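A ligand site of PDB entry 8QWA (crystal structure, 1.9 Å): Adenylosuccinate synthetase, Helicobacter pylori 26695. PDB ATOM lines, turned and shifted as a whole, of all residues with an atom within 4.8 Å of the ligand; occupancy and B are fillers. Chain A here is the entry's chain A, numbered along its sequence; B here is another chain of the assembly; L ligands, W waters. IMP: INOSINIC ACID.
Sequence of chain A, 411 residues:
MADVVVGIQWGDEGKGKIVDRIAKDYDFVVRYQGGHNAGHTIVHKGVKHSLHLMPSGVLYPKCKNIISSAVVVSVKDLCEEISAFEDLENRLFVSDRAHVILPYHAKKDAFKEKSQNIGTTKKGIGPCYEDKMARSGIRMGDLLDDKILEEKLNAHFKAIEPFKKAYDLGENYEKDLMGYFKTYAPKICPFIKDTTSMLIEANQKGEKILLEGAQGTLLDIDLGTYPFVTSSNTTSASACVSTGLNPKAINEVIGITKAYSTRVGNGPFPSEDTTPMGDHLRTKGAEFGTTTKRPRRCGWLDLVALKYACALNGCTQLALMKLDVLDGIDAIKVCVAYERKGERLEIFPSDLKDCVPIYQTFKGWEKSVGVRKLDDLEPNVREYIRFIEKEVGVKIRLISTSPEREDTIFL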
ATOM      1  N   TRP A  10      -9.778  -5.687 -18.877  1.00  0.00           N
ATOM      2  CA  TRP A  10      -8.568  -6.164 -18.222  1.00  0.00           C
ATOM      3  C   TRP A  10      -8.419  -7.667 -18.357  1.00  0.00           C
ATOM      4  O   TRP A  10      -8.104  -8.371 -17.406  1.00  0.00           O
ATOM      5  CB  TRP A  10      -8.544  -5.828 -16.709  1.00  0.00           C
ATOM      6  CG  TRP A  10      -8.431  -4.394 -16.305  1.00  0.00           C
ATOM      7  CD1 TRP A  10      -7.295  -3.670 -16.114  1.00  0.00           C
ATOM      8  CD2 TRP A  10      -9.520  -3.535 -15.921  1.00  0.00           C
ATOM      9  NE1 TRP A  10      -7.600  -2.421 -15.631  1.00  0.00           N
ATOM     10  CE2 TRP A  10      -8.953  -2.300 -15.503  1.00  0.00           C
ATOM     11  CE3 TRP A  10     -10.909  -3.683 -15.874  1.00  0.00           C
ATOM     12  CZ2 TRP A  10      -9.727  -1.245 -15.033  1.00  0.00           C
ATOM     13  CZ3 TRP A  10     -11.661  -2.617 -15.419  1.00  0.00           C
ATOM     14  CH2 TRP A  10     -11.091  -1.430 -15.016  1.00  0.00           C
ATOM     15  N   GLY A  11      -8.613  -8.178 -19.568  1.00  0.00           N
ATOM     16  CA  GLY A  11      -8.461  -9.595 -19.815  1.00  0.00           C
ATOM     17  C   GLY A  11      -9.727 -10.386 -19.459  1.00  0.00           C
ATOM     18  O   GLY A  11     -10.696  -9.826 -18.975  1.00  0.00           O
ATOM     19  N   ASP A  12      -9.720 -11.680 -19.806  1.00  0.00           N
ATOM     20  CA  ASP A  12     -10.800 -12.580 -19.458  1.00  0.00           C
ATOM     21  C   ASP A  12     -12.120 -12.173 -20.108  1.00  0.00           C
ATOM     22  O   ASP A  12     -13.176 -12.439 -19.535  1.00  0.00           O
ATOM     23  CB  ASP A  12     -10.969 -12.720 -17.941  1.00  0.00           C
ATOM     24  CG  ASP A  12      -9.675 -13.026 -17.190  1.00  0.00           C
ATOM     25  OD1 ASP A  12      -8.835 -13.739 -17.795  1.00  0.00           O
ATOM     26  OD2 ASP A  12      -9.491 -12.518 -16.050  1.00  0.00           O
ATOM     27  N   ASN A  37       0.806 -16.316 -19.426  1.00  0.00           N
ATOM     28  CA  ASN A  37      -0.041 -15.586 -18.510  1.00  0.00           C
ATOM     29  C   ASN A  37      -1.482 -15.640 -19.027  1.00  0.00           C
ATOM     30  O   ASN A  37      -2.413 -15.681 -18.207  1.00  0.00           O
ATOM     31  CB  ASN A  37       0.471 -14.176 -18.238  1.00  0.00           C
ATOM     32  CG  ASN A  37       0.803 -13.360 -19.473  1.00  0.00           C
ATOM     33  OD1 ASN A  37       0.870 -13.893 -20.586  1.00  0.00           O
ATOM     34  ND2 ASN A  37       1.058 -12.071 -19.274  1.00  0.00           N
ATOM     35  N   ALA A  38      -1.657 -15.686 -20.354  1.00  0.00           N
ATOM     36  CA  ALA A  38      -2.961 -15.860 -20.986  1.00  0.00           C
ATOM     37  C   ALA A  38      -3.553 -17.233 -20.659  1.00  0.00           C
ATOM     38  O   ALA A  38      -2.770 -18.160 -20.447  1.00  0.00           O
ATOM     39  CB  ALA A  38      -2.802 -15.704 -22.492  1.00  0.00           C
ATOM     40  N   GLY A  39      -4.900 -17.347 -20.730  1.00  0.00           N
ATOM     41  CA  GLY A  39      -5.647 -18.603 -20.588  1.00  0.00           C
ATOM     42  C   GLY A  39      -6.858 -18.691 -21.548  1.00  0.00           C
ATOM     43  O   GLY A  39      -7.947 -18.957 -21.119  1.00  0.00           O
ATOM     44  N   ILE A 118       1.859  -6.184  -7.348  1.00  0.00           N
ATOM     45  CA  ILE A 118       1.001  -5.858  -8.485  1.00  0.00           C
ATOM     46  C   ILE A 118      -0.128  -6.876  -8.602  1.00  0.00           C
ATOM     47  O   ILE A 118      -1.231  -6.544  -9.028  1.00  0.00           O
ATOM     48  CB  ILE A 118       1.876  -5.774  -9.748  1.00  0.00           C
ATOM     49  CG1 ILE A 118       2.716  -4.498  -9.711  1.00  0.00           C
ATOM     50  CG2 ILE A 118       1.039  -5.894 -11.019  1.00  0.00           C
ATOM     51  CD1 ILE A 118       3.907  -4.522 -10.627  1.00  0.00           C
ATOM     52  N   GLY A 119       0.172  -8.146  -8.313  1.00  0.00           N
ATOM     53  CA  GLY A 119      -0.733  -9.252  -8.581  1.00  0.00           C
ATOM     54  C   GLY A 119      -0.420  -9.894  -9.935  1.00  0.00           C
ATOM     55  O   GLY A 119      -1.340 -10.196 -10.714  1.00  0.00           O
ATOM     56  N   THR A 120       0.877 -10.053 -10.238  1.00  0.00           N
ATOM     57  CA  THR A 120       1.268 -10.675 -11.491  1.00  0.00           C
ATOM     58  C   THR A 120       0.855 -12.134 -11.489  1.00  0.00           C
ATOM     59  O   THR A 120       0.463 -12.710 -10.445  1.00  0.00           O
ATOM     60  CB  THR A 120       2.759 -10.549 -11.810  1.00  0.00           C
ATOM     61  OG1 THR A 120       3.494 -11.452 -10.988  1.00  0.00           O
ATOM     62  CG2 THR A 120       3.280  -9.142 -11.730  1.00  0.00           C
ATOM     63  N   THR A 121       0.977 -12.765 -12.659  1.00  0.00           N
ATOM     64  CA  THR A 121       0.753 -14.191 -12.761  1.00  0.00           C
ATOM     65  C   THR A 121       1.917 -15.012 -12.198  1.00  0.00           C
ATOM     66  O   THR A 121       1.786 -16.225 -12.189  1.00  0.00           O
ATOM     67  CB  THR A 121       0.364 -14.656 -14.171  1.00  0.00           C
ATOM     68  OG1 THR A 121       1.460 -14.490 -15.065  1.00  0.00           O
ATOM     69  CG2 THR A 121      -0.900 -13.993 -14.681  1.00  0.00           C
ATOM     70  N   LYS A 122       3.000 -14.366 -11.736  1.00  0.00           N
ATOM     71  CA  LYS A 122       4.205 -15.025 -11.242  1.00  0.00           C
ATOM     72  C   LYS A 122       4.781 -16.026 -12.248  1.00  0.00           C
ATOM     73  O   LYS A 122       5.387 -17.051 -11.865  1.00  0.00           O
ATOM     74  CB  LYS A 122       3.925 -15.627  -9.862  1.00  0.00           C
ATOM     75  CG  LYS A 122       3.662 -14.553  -8.790  1.00  0.00           C
ATOM     76  CD  LYS A 122       3.542 -15.010  -7.330  1.00  0.00           C
ATOM     77  CE  LYS A 122       2.151 -15.503  -7.018  1.00  0.00           C
ATOM     78  NZ  LYS A 122       2.035 -16.191  -5.727  1.00  0.00           N
ATOM     79  N   ILE A 125       6.815 -13.143 -16.755  1.00  0.00           N
ATOM     80  CA  ILE A 125       6.546 -12.379 -17.977  1.00  0.00           C
ATOM     81  C   ILE A 125       7.357 -11.071 -17.973  1.00  0.00           C
ATOM     82  O   ILE A 125       8.074 -10.758 -18.929  1.00  0.00           O
ATOM     83  CB  ILE A 125       5.028 -12.109 -18.096  1.00  0.00           C
ATOM     84  CG1 ILE A 125       4.189 -13.427 -18.106  1.00  0.00           C
ATOM     85  CG2 ILE A 125       4.708 -11.234 -19.326  1.00  0.00           C
ATOM     86  CD1 ILE A 125       4.421 -14.364 -19.275  1.00  0.00           C
ATOM     87  N   GLY A 126       7.159 -10.274 -16.921  1.00  0.00           N
ATOM     88  CA  GLY A 126       7.785  -8.988 -16.800  1.00  0.00           C
ATOM     89  C   GLY A 126       9.298  -9.092 -16.895  1.00  0.00           C
ATOM     90  O   GLY A 126       9.951  -8.419 -17.678  1.00  0.00           O
ATOM     91  N   GLN A 215      -4.339 -10.668 -22.785  1.00  0.00           N
ATOM     92  CA  GLN A 215      -4.656  -9.705 -21.737  1.00  0.00           C
ATOM     93  C   GLN A 215      -5.760  -8.803 -22.222  1.00  0.00           C
ATOM     94  O   GLN A 215      -6.748  -9.293 -22.773  1.00  0.00           O
ATOM     95  CB  GLN A 215      -3.395  -8.975 -21.279  1.00  0.00           C
ATOM     96  CG  GLN A 215      -2.446  -9.884 -20.513  1.00  0.00           C
ATOM     97  CD  GLN A 215      -1.622 -10.776 -21.387  1.00  0.00           C
ATOM     98  OE1 GLN A 215      -0.968 -10.343 -22.340  1.00  0.00           O
ATOM     99  NE2 GLN A 215      -1.649 -12.058 -21.073  1.00  0.00           N
ATOM    100  N   LEU A 219      -4.734  -3.289 -19.501  1.00  0.00           N
ATOM    101  CA  LEU A 219      -3.495  -3.876 -19.016  1.00  0.00           C
ATOM    102  C   LEU A 219      -2.289  -3.457 -19.868  1.00  0.00           C
ATOM    103  O   LEU A 219      -1.167  -3.906 -19.619  1.00  0.00           O
ATOM    104  CB  LEU A 219      -3.650  -5.399 -19.003  1.00  0.00           C
ATOM    105  CG  LEU A 219      -4.517  -5.921 -17.862  1.00  0.00           C
ATOM    106  CD1 LEU A 219      -4.751  -7.416 -18.027  1.00  0.00           C
ATOM    107  CD2 LEU A 219      -3.962  -5.591 -16.479  1.00  0.00           C
ATOM    108  N   VAL A 229      -0.620  -3.395 -14.678  1.00  0.00           N
ATOM    109  CA  VAL A 229      -0.628  -3.728 -16.098  1.00  0.00           C
ATOM    110  C   VAL A 229       0.298  -4.917 -16.345  1.00  0.00           C
ATOM    111  O   VAL A 229       1.113  -5.244 -15.488  1.00  0.00           O
ATOM    112  CB  VAL A 229      -0.137  -2.505 -16.894  1.00  0.00           C
ATOM    113  CG1 VAL A 229      -1.121  -1.341 -16.817  1.00  0.00           C
ATOM    114  CG2 VAL A 229       1.245  -2.011 -16.451  1.00  0.00           C
ATOM    115  N   THR A 230       0.218  -5.503 -17.549  1.00  0.00           N
ATOM    116  CA  THR A 230       1.238  -6.396 -18.031  1.00  0.00           C
ATOM    117  C   THR A 230       2.324  -5.596 -18.751  1.00  0.00           C
ATOM    118  O   THR A 230       2.172  -4.421 -19.080  1.00  0.00           O
ATOM    119  CB  THR A 230       0.556  -7.494 -18.885  1.00  0.00           C
ATOM    120  OG1 THR A 230       1.446  -8.589 -19.039  1.00  0.00           O
ATOM    121  CG2 THR A 230       0.054  -7.014 -20.242  1.00  0.00           C
ATOM    122  N   ARG A 263     -11.349  -7.721 -12.893  1.00  0.00           N
ATOM    123  CA  ARG A 263      -9.895  -7.648 -12.842  1.00  0.00           C
ATOM    124  C   ARG A 263      -9.428  -8.811 -11.989  1.00  0.00           C
ATOM    125  O   ARG A 263     -10.148  -9.259 -11.066  1.00  0.00           O
ATOM    126  CB  ARG A 263      -9.364  -6.462 -12.027  1.00  0.00           C
ATOM    127  CG  ARG A 263      -9.459  -5.161 -12.776  1.00  0.00           C
ATOM    128  CD  ARG A 263      -8.557  -4.123 -12.142  1.00  0.00           C
ATOM    129  NE  ARG A 263      -7.172  -4.375 -12.501  1.00  0.00           N
ATOM    130  CZ  ARG A 263      -6.266  -3.514 -12.836  1.00  0.00           C
ATOM    131  NH1 ARG A 263      -6.486  -2.236 -12.624  1.00  0.00           N
ATOM    132  NH2 ARG A 263      -5.122  -3.976 -13.305  1.00  0.00           N
ATOM    133  N   VAL A 264      -8.248  -9.318 -12.316  1.00  0.00           N
ATOM    134  CA  VAL A 264      -7.589 -10.256 -11.428  1.00  0.00           C
ATOM    135  C   VAL A 264      -6.213  -9.656 -11.149  1.00  0.00           C
ATOM    136  O   VAL A 264      -5.525  -9.190 -12.054  1.00  0.00           O
ATOM    137  CB  VAL A 264      -7.527 -11.705 -11.938  1.00  0.00           C
ATOM    138  CG1 VAL A 264      -6.786 -11.842 -13.256  1.00  0.00           C
ATOM    139  CG2 VAL A 264      -6.934 -12.649 -10.881  1.00  0.00           C
ATOM    140  N   GLY A 265      -5.848  -9.648  -9.866  1.00  0.00           N
ATOM    141  CA  GLY A 265      -4.733  -8.829  -9.410  1.00  0.00           C
ATOM    142  C   GLY A 265      -5.191  -7.492  -8.872  1.00  0.00           C
ATOM    143  O   GLY A 265      -6.388  -7.188  -8.848  1.00  0.00           O
ATOM    144  N   ASN A 266      -4.208  -6.721  -8.401  1.00  0.00           N
ATOM    145  CA  ASN A 266      -4.445  -5.443  -7.768  1.00  0.00           C
ATOM    146  C   ASN A 266      -4.660  -4.354  -8.830  1.00  0.00           C
ATOM    147  O   ASN A 266      -4.476  -4.563 -10.031  1.00  0.00           O
ATOM    148  CB  ASN A 266      -3.318  -5.126  -6.798  1.00  0.00           C
ATOM    149  CG  ASN A 266      -3.414  -6.008  -5.574  1.00  0.00           C
ATOM    150  OD1 ASN A 266      -4.526  -6.219  -5.046  1.00  0.00           O
ATOM    151  ND2 ASN A 266      -2.276  -6.494  -5.099  1.00  0.00           N
ATOM    152  N   ARG A 294      -7.004 -17.812  -9.781  1.00  0.00           N
ATOM    153  CA  ARG A 294      -7.271 -16.772  -8.819  1.00  0.00           C
ATOM    154  C   ARG A 294      -8.652 -16.218  -9.106  1.00  0.00           C
ATOM    155  O   ARG A 294      -9.023 -16.043 -10.269  1.00  0.00           O
ATOM    156  CB  ARG A 294      -6.237 -15.665  -8.996  1.00  0.00           C
ATOM    157  CG  ARG A 294      -4.799 -15.992  -8.630  1.00  0.00           C
ATOM    158  CD  ARG A 294      -3.875 -14.799  -8.893  1.00  0.00           C
ATOM    159  NE  ARG A 294      -3.757 -14.551 -10.340  1.00  0.00           N
ATOM    160  CZ  ARG A 294      -3.407 -13.376 -10.864  1.00  0.00           C
ATOM    161  NH1 ARG A 294      -3.093 -12.348 -10.087  1.00  0.00           N
ATOM    162  NH2 ARG A 294      -3.376 -13.239 -12.179  1.00  0.00           N
ATOM    163  N   ARG A 296     -11.654 -13.677  -9.751  1.00  0.00           N
ATOM    164  CA  ARG A 296     -11.661 -12.326 -10.283  1.00  0.00           C
ATOM    165  C   ARG A 296     -12.488 -11.396  -9.370  1.00  0.00           C
ATOM    166  O   ARG A 296     -13.546 -11.767  -8.862  1.00  0.00           O
ATOM    167  CB  ARG A 296     -12.268 -12.347 -11.701  1.00  0.00           C
ATOM    168  CG  ARG A 296     -11.325 -12.693 -12.856  1.00  0.00           C
ATOM    169  CD  ARG A 296     -10.485 -13.952 -12.698  1.00  0.00           C
ATOM    170  NE  ARG A 296      -9.583 -14.047 -13.858  1.00  0.00           N
ATOM    171  CZ  ARG A 296      -8.580 -14.908 -13.924  1.00  0.00           C
ATOM    172  NH1 ARG A 296      -8.293 -15.664 -12.860  1.00  0.00           N
ATOM    173  NH2 ARG A 296      -7.841 -14.985 -15.014  1.00  0.00           N
ATOM    174  N   ARG B 135       7.757  -2.307 -14.061  1.00  0.00           N
ATOM    175  CA  ARG B 135       6.652  -1.555 -13.521  1.00  0.00           C
ATOM    176  C   ARG B 135       7.080  -0.919 -12.204  1.00  0.00           C
ATOM    177  O   ARG B 135       6.226  -0.555 -11.405  1.00  0.00           O
ATOM    178  CB  ARG B 135       5.331  -2.319 -13.443  1.00  0.00           C
ATOM    179  CG  ARG B 135       4.785  -2.663 -14.824  1.00  0.00           C
ATOM    180  CD  ARG B 135       4.102  -3.998 -14.833  1.00  0.00           C
ATOM    181  NE  ARG B 135       5.065  -5.100 -14.641  1.00  0.00           N
ATOM    182  CZ  ARG B 135       4.774  -6.400 -14.591  1.00  0.00           C
ATOM    183  NH1 ARG B 135       3.545  -6.849 -14.792  1.00  0.00           N
ATOM    184  NH2 ARG B 135       5.721  -7.293 -14.383  1.00  0.00           N
HETATM  185  P   IMP L   1       1.769 -10.435 -15.678  1.00  0.00           P
HETATM  186  O1P IMP L   1       1.924 -11.857 -15.167  1.00  0.00           O
HETATM  187  O2P IMP L   1       1.276 -10.344 -17.106  1.00  0.00           O
HETATM  188  O3P IMP L   1       2.995  -9.567 -15.417  1.00  0.00           O
HETATM  189  O5' IMP L   1       0.539  -9.862 -14.770  1.00  0.00           O
HETATM  190  C5' IMP L   1       0.301  -8.409 -14.759  1.00  0.00           C
HETATM  191  C4' IMP L   1      -1.181  -8.096 -14.647  1.00  0.00           C
HETATM  192  O4' IMP L   1      -1.906  -8.599 -15.807  1.00  0.00           O
HETATM  193  C3' IMP L   1      -1.926  -8.680 -13.450  1.00  0.00           C
HETATM  194  O3' IMP L   1      -2.968  -7.826 -13.014  1.00  0.00           O
HETATM  195  C2' IMP L   1      -2.413 -10.021 -13.987  1.00  0.00           C
HETATM  196  O2' IMP L   1      -3.413 -10.604 -13.149  1.00  0.00           O
HETATM  197  C1' IMP L   1      -2.864  -9.535 -15.372  1.00  0.00           C
HETATM  198  N9  IMP L   1      -2.980 -10.569 -16.377  1.00  0.00           N
HETATM  199  C8  IMP L   1      -2.022 -11.177 -17.141  1.00  0.00           C
HETATM  200  N7  IMP L   1      -2.514 -12.032 -18.004  1.00  0.00           N
HETATM  201  C5  IMP L   1      -3.891 -12.007 -17.751  1.00  0.00           C
HETATM  202  C6  IMP L   1      -4.959 -12.721 -18.362  1.00  0.00           C
HETATM  203  O6  IMP L   1      -4.928 -13.547 -19.274  1.00  0.00           O
HETATM  204  N1  IMP L   1      -6.184 -12.372 -17.753  1.00  0.00           N
HETATM  205  C2  IMP L   1      -6.355 -11.430 -16.789  1.00  0.00           C
HETATM  206  N3  IMP L   1      -5.372 -10.760 -16.226  1.00  0.00           N
HETATM  207  C4  IMP L   1      -4.176 -11.088 -16.768  1.00  0.00           C
HETATM  208  O   HOH W   1      -5.018 -13.219 -22.159  1.00  0.00           O
HETATM  209  O   HOH W   2      -2.506  -5.794 -11.462  1.00  0.00           O
HETATM  210  O   HOH W   3       4.335 -13.198 -14.870  1.00  0.00           O
HETATM  211  O   HOH W   4      -7.401 -13.095 -20.936  1.00  0.00           O
HETATM  212  O   HOH W   5      -6.996  -8.672 -15.007  1.00  0.00           O
HETATM  213  O   HOH W   6      -5.878  -6.818 -13.415  1.00  0.00           O
HETATM  214  O   HOH W   7       5.422 -10.161 -14.516  1.00  0.00           O
HETATM  215  O   HOH W   8       4.339  -8.578 -17.529  1.00  0.00           O
HETATM  216  O   HOH W   9      -4.501 -15.030 -16.505  1.00  0.00           O
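OG1 of Thr 230 lies within hydrogen-bond range of O2P of the ligand, 2.6 Å away. The side-chain hydroxyl (OG1) of Thr 121 is in hydrogen-bond range of an oxygen (O1P) of the ligand, 2.7 Å away. The guanidinium group (NH2) of Arg 294 sits at hydrogen-bond distance from an oxygen (O2') of the ligand (2.8 Å). N7 of the ligand sits at hydrogen-bond distance from NE2 of Gln 215 (3.2 Å). ND2 of Asn 37 lies within hydrogen-bond range of O2P of the ligand. O of Val 264 sits at hydrogen-bond distance from O2' of the ligand, at 2.8 Å. N of Thr 121 is in hydrogen-bond range of O1P of the ligand (2.8 Å). An oxygen (O3P) of the ligand is in salt-bridge range of the guanidinium group (NH1) of Arg 135 of chain B. OD1 of Asp 12 is in hydrogen-bond range of N1 of the ligand, at 3.0 Å. An oxygen (O2') of the ligand sits close to the backbone carbonyl oxygen (O) of Gly 119 (3.2 Å).
O of Arg 294 is in hydrogen-bond range of NH1 of Arg 296, at 2.7 Å. The side-chain amide oxygen of Asn 37 is in hydrogen-bond range of the side-chain amide nitrogen of Gln 215 (3.2 Å). The guanidinium group (NH1) of Arg 294 lies within hydrogen-bond range of the backbone carbonyl oxygen (O) of Gly 119 (2.8 Å). The guanidinium group of Arg 135 of chain B is in hydrogen-bond range of the backbone carbonyl oxygen of Val 229 (3.0 Å). N of Thr 230 sits at hydrogen-bond distance from O of Leu 219. OD2 of Asp 12 lies within salt-bridge range of NE of Arg 296. N of Lys 122 sits at hydrogen-bond distance from OG1 of Thr 120 (3.0 Å).
Trp 10 touches the ligand (O to C2, 3.6 Å). Ala 38 touches the ligand. Thr 120 touches the ligand (CA to O5', 3.5 Å). Leu 219 touches the ligand (CD2 to O4', 3.7 Å). Val 229 touches the ligand. Within 4 Å of the ligand: Trp 10, Asp 12, Asn 37, Ala 38, Gly 119, Thr 120, Thr 121, Gln 215, Leu 219, Val 229, Thr 230, Val 264, Arg 294 and Arg 135 of chain B.
Water W2 lies within hydrogen-bond range of an oxygen (O3') of the ligand (2.6 Å), the backbone carbonyl oxygen of Asn 266 (2.7 Å) and the backbone carbonyl oxygen of Ile 118 (2.8 Å). Water W8 lies within hydrogen-bond range of an oxygen (O3P) of the ligand, the side-chain hydroxyl of Thr 230, the guanidinium group of Arg 135 of chain B and the backbone NH of Gly 126. Water W3 lies within hydrogen-bond range of O1P of the ligand (2.8 Å), N of Ile 125 (3.1 Å) and OG1 of Thr 121 (3.2 Å). Water W1 lies within hydrogen-bond range of N of Gln 215 (2.7 Å) and O6 of the ligand (2.9 Å). Water W5 lies within hydrogen-bond range of the backbone carbonyl oxygen (O) of Trp 10 (2.7 Å), a nitrogen (N3) of the ligand (2.9 Å) and the backbone NH (N) of Val 264 (3.0 Å). Water W4 bridges the backbone NH of Asp 12 (2.9 Å) and an oxygen (O6) of the ligand (3.0 Å).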
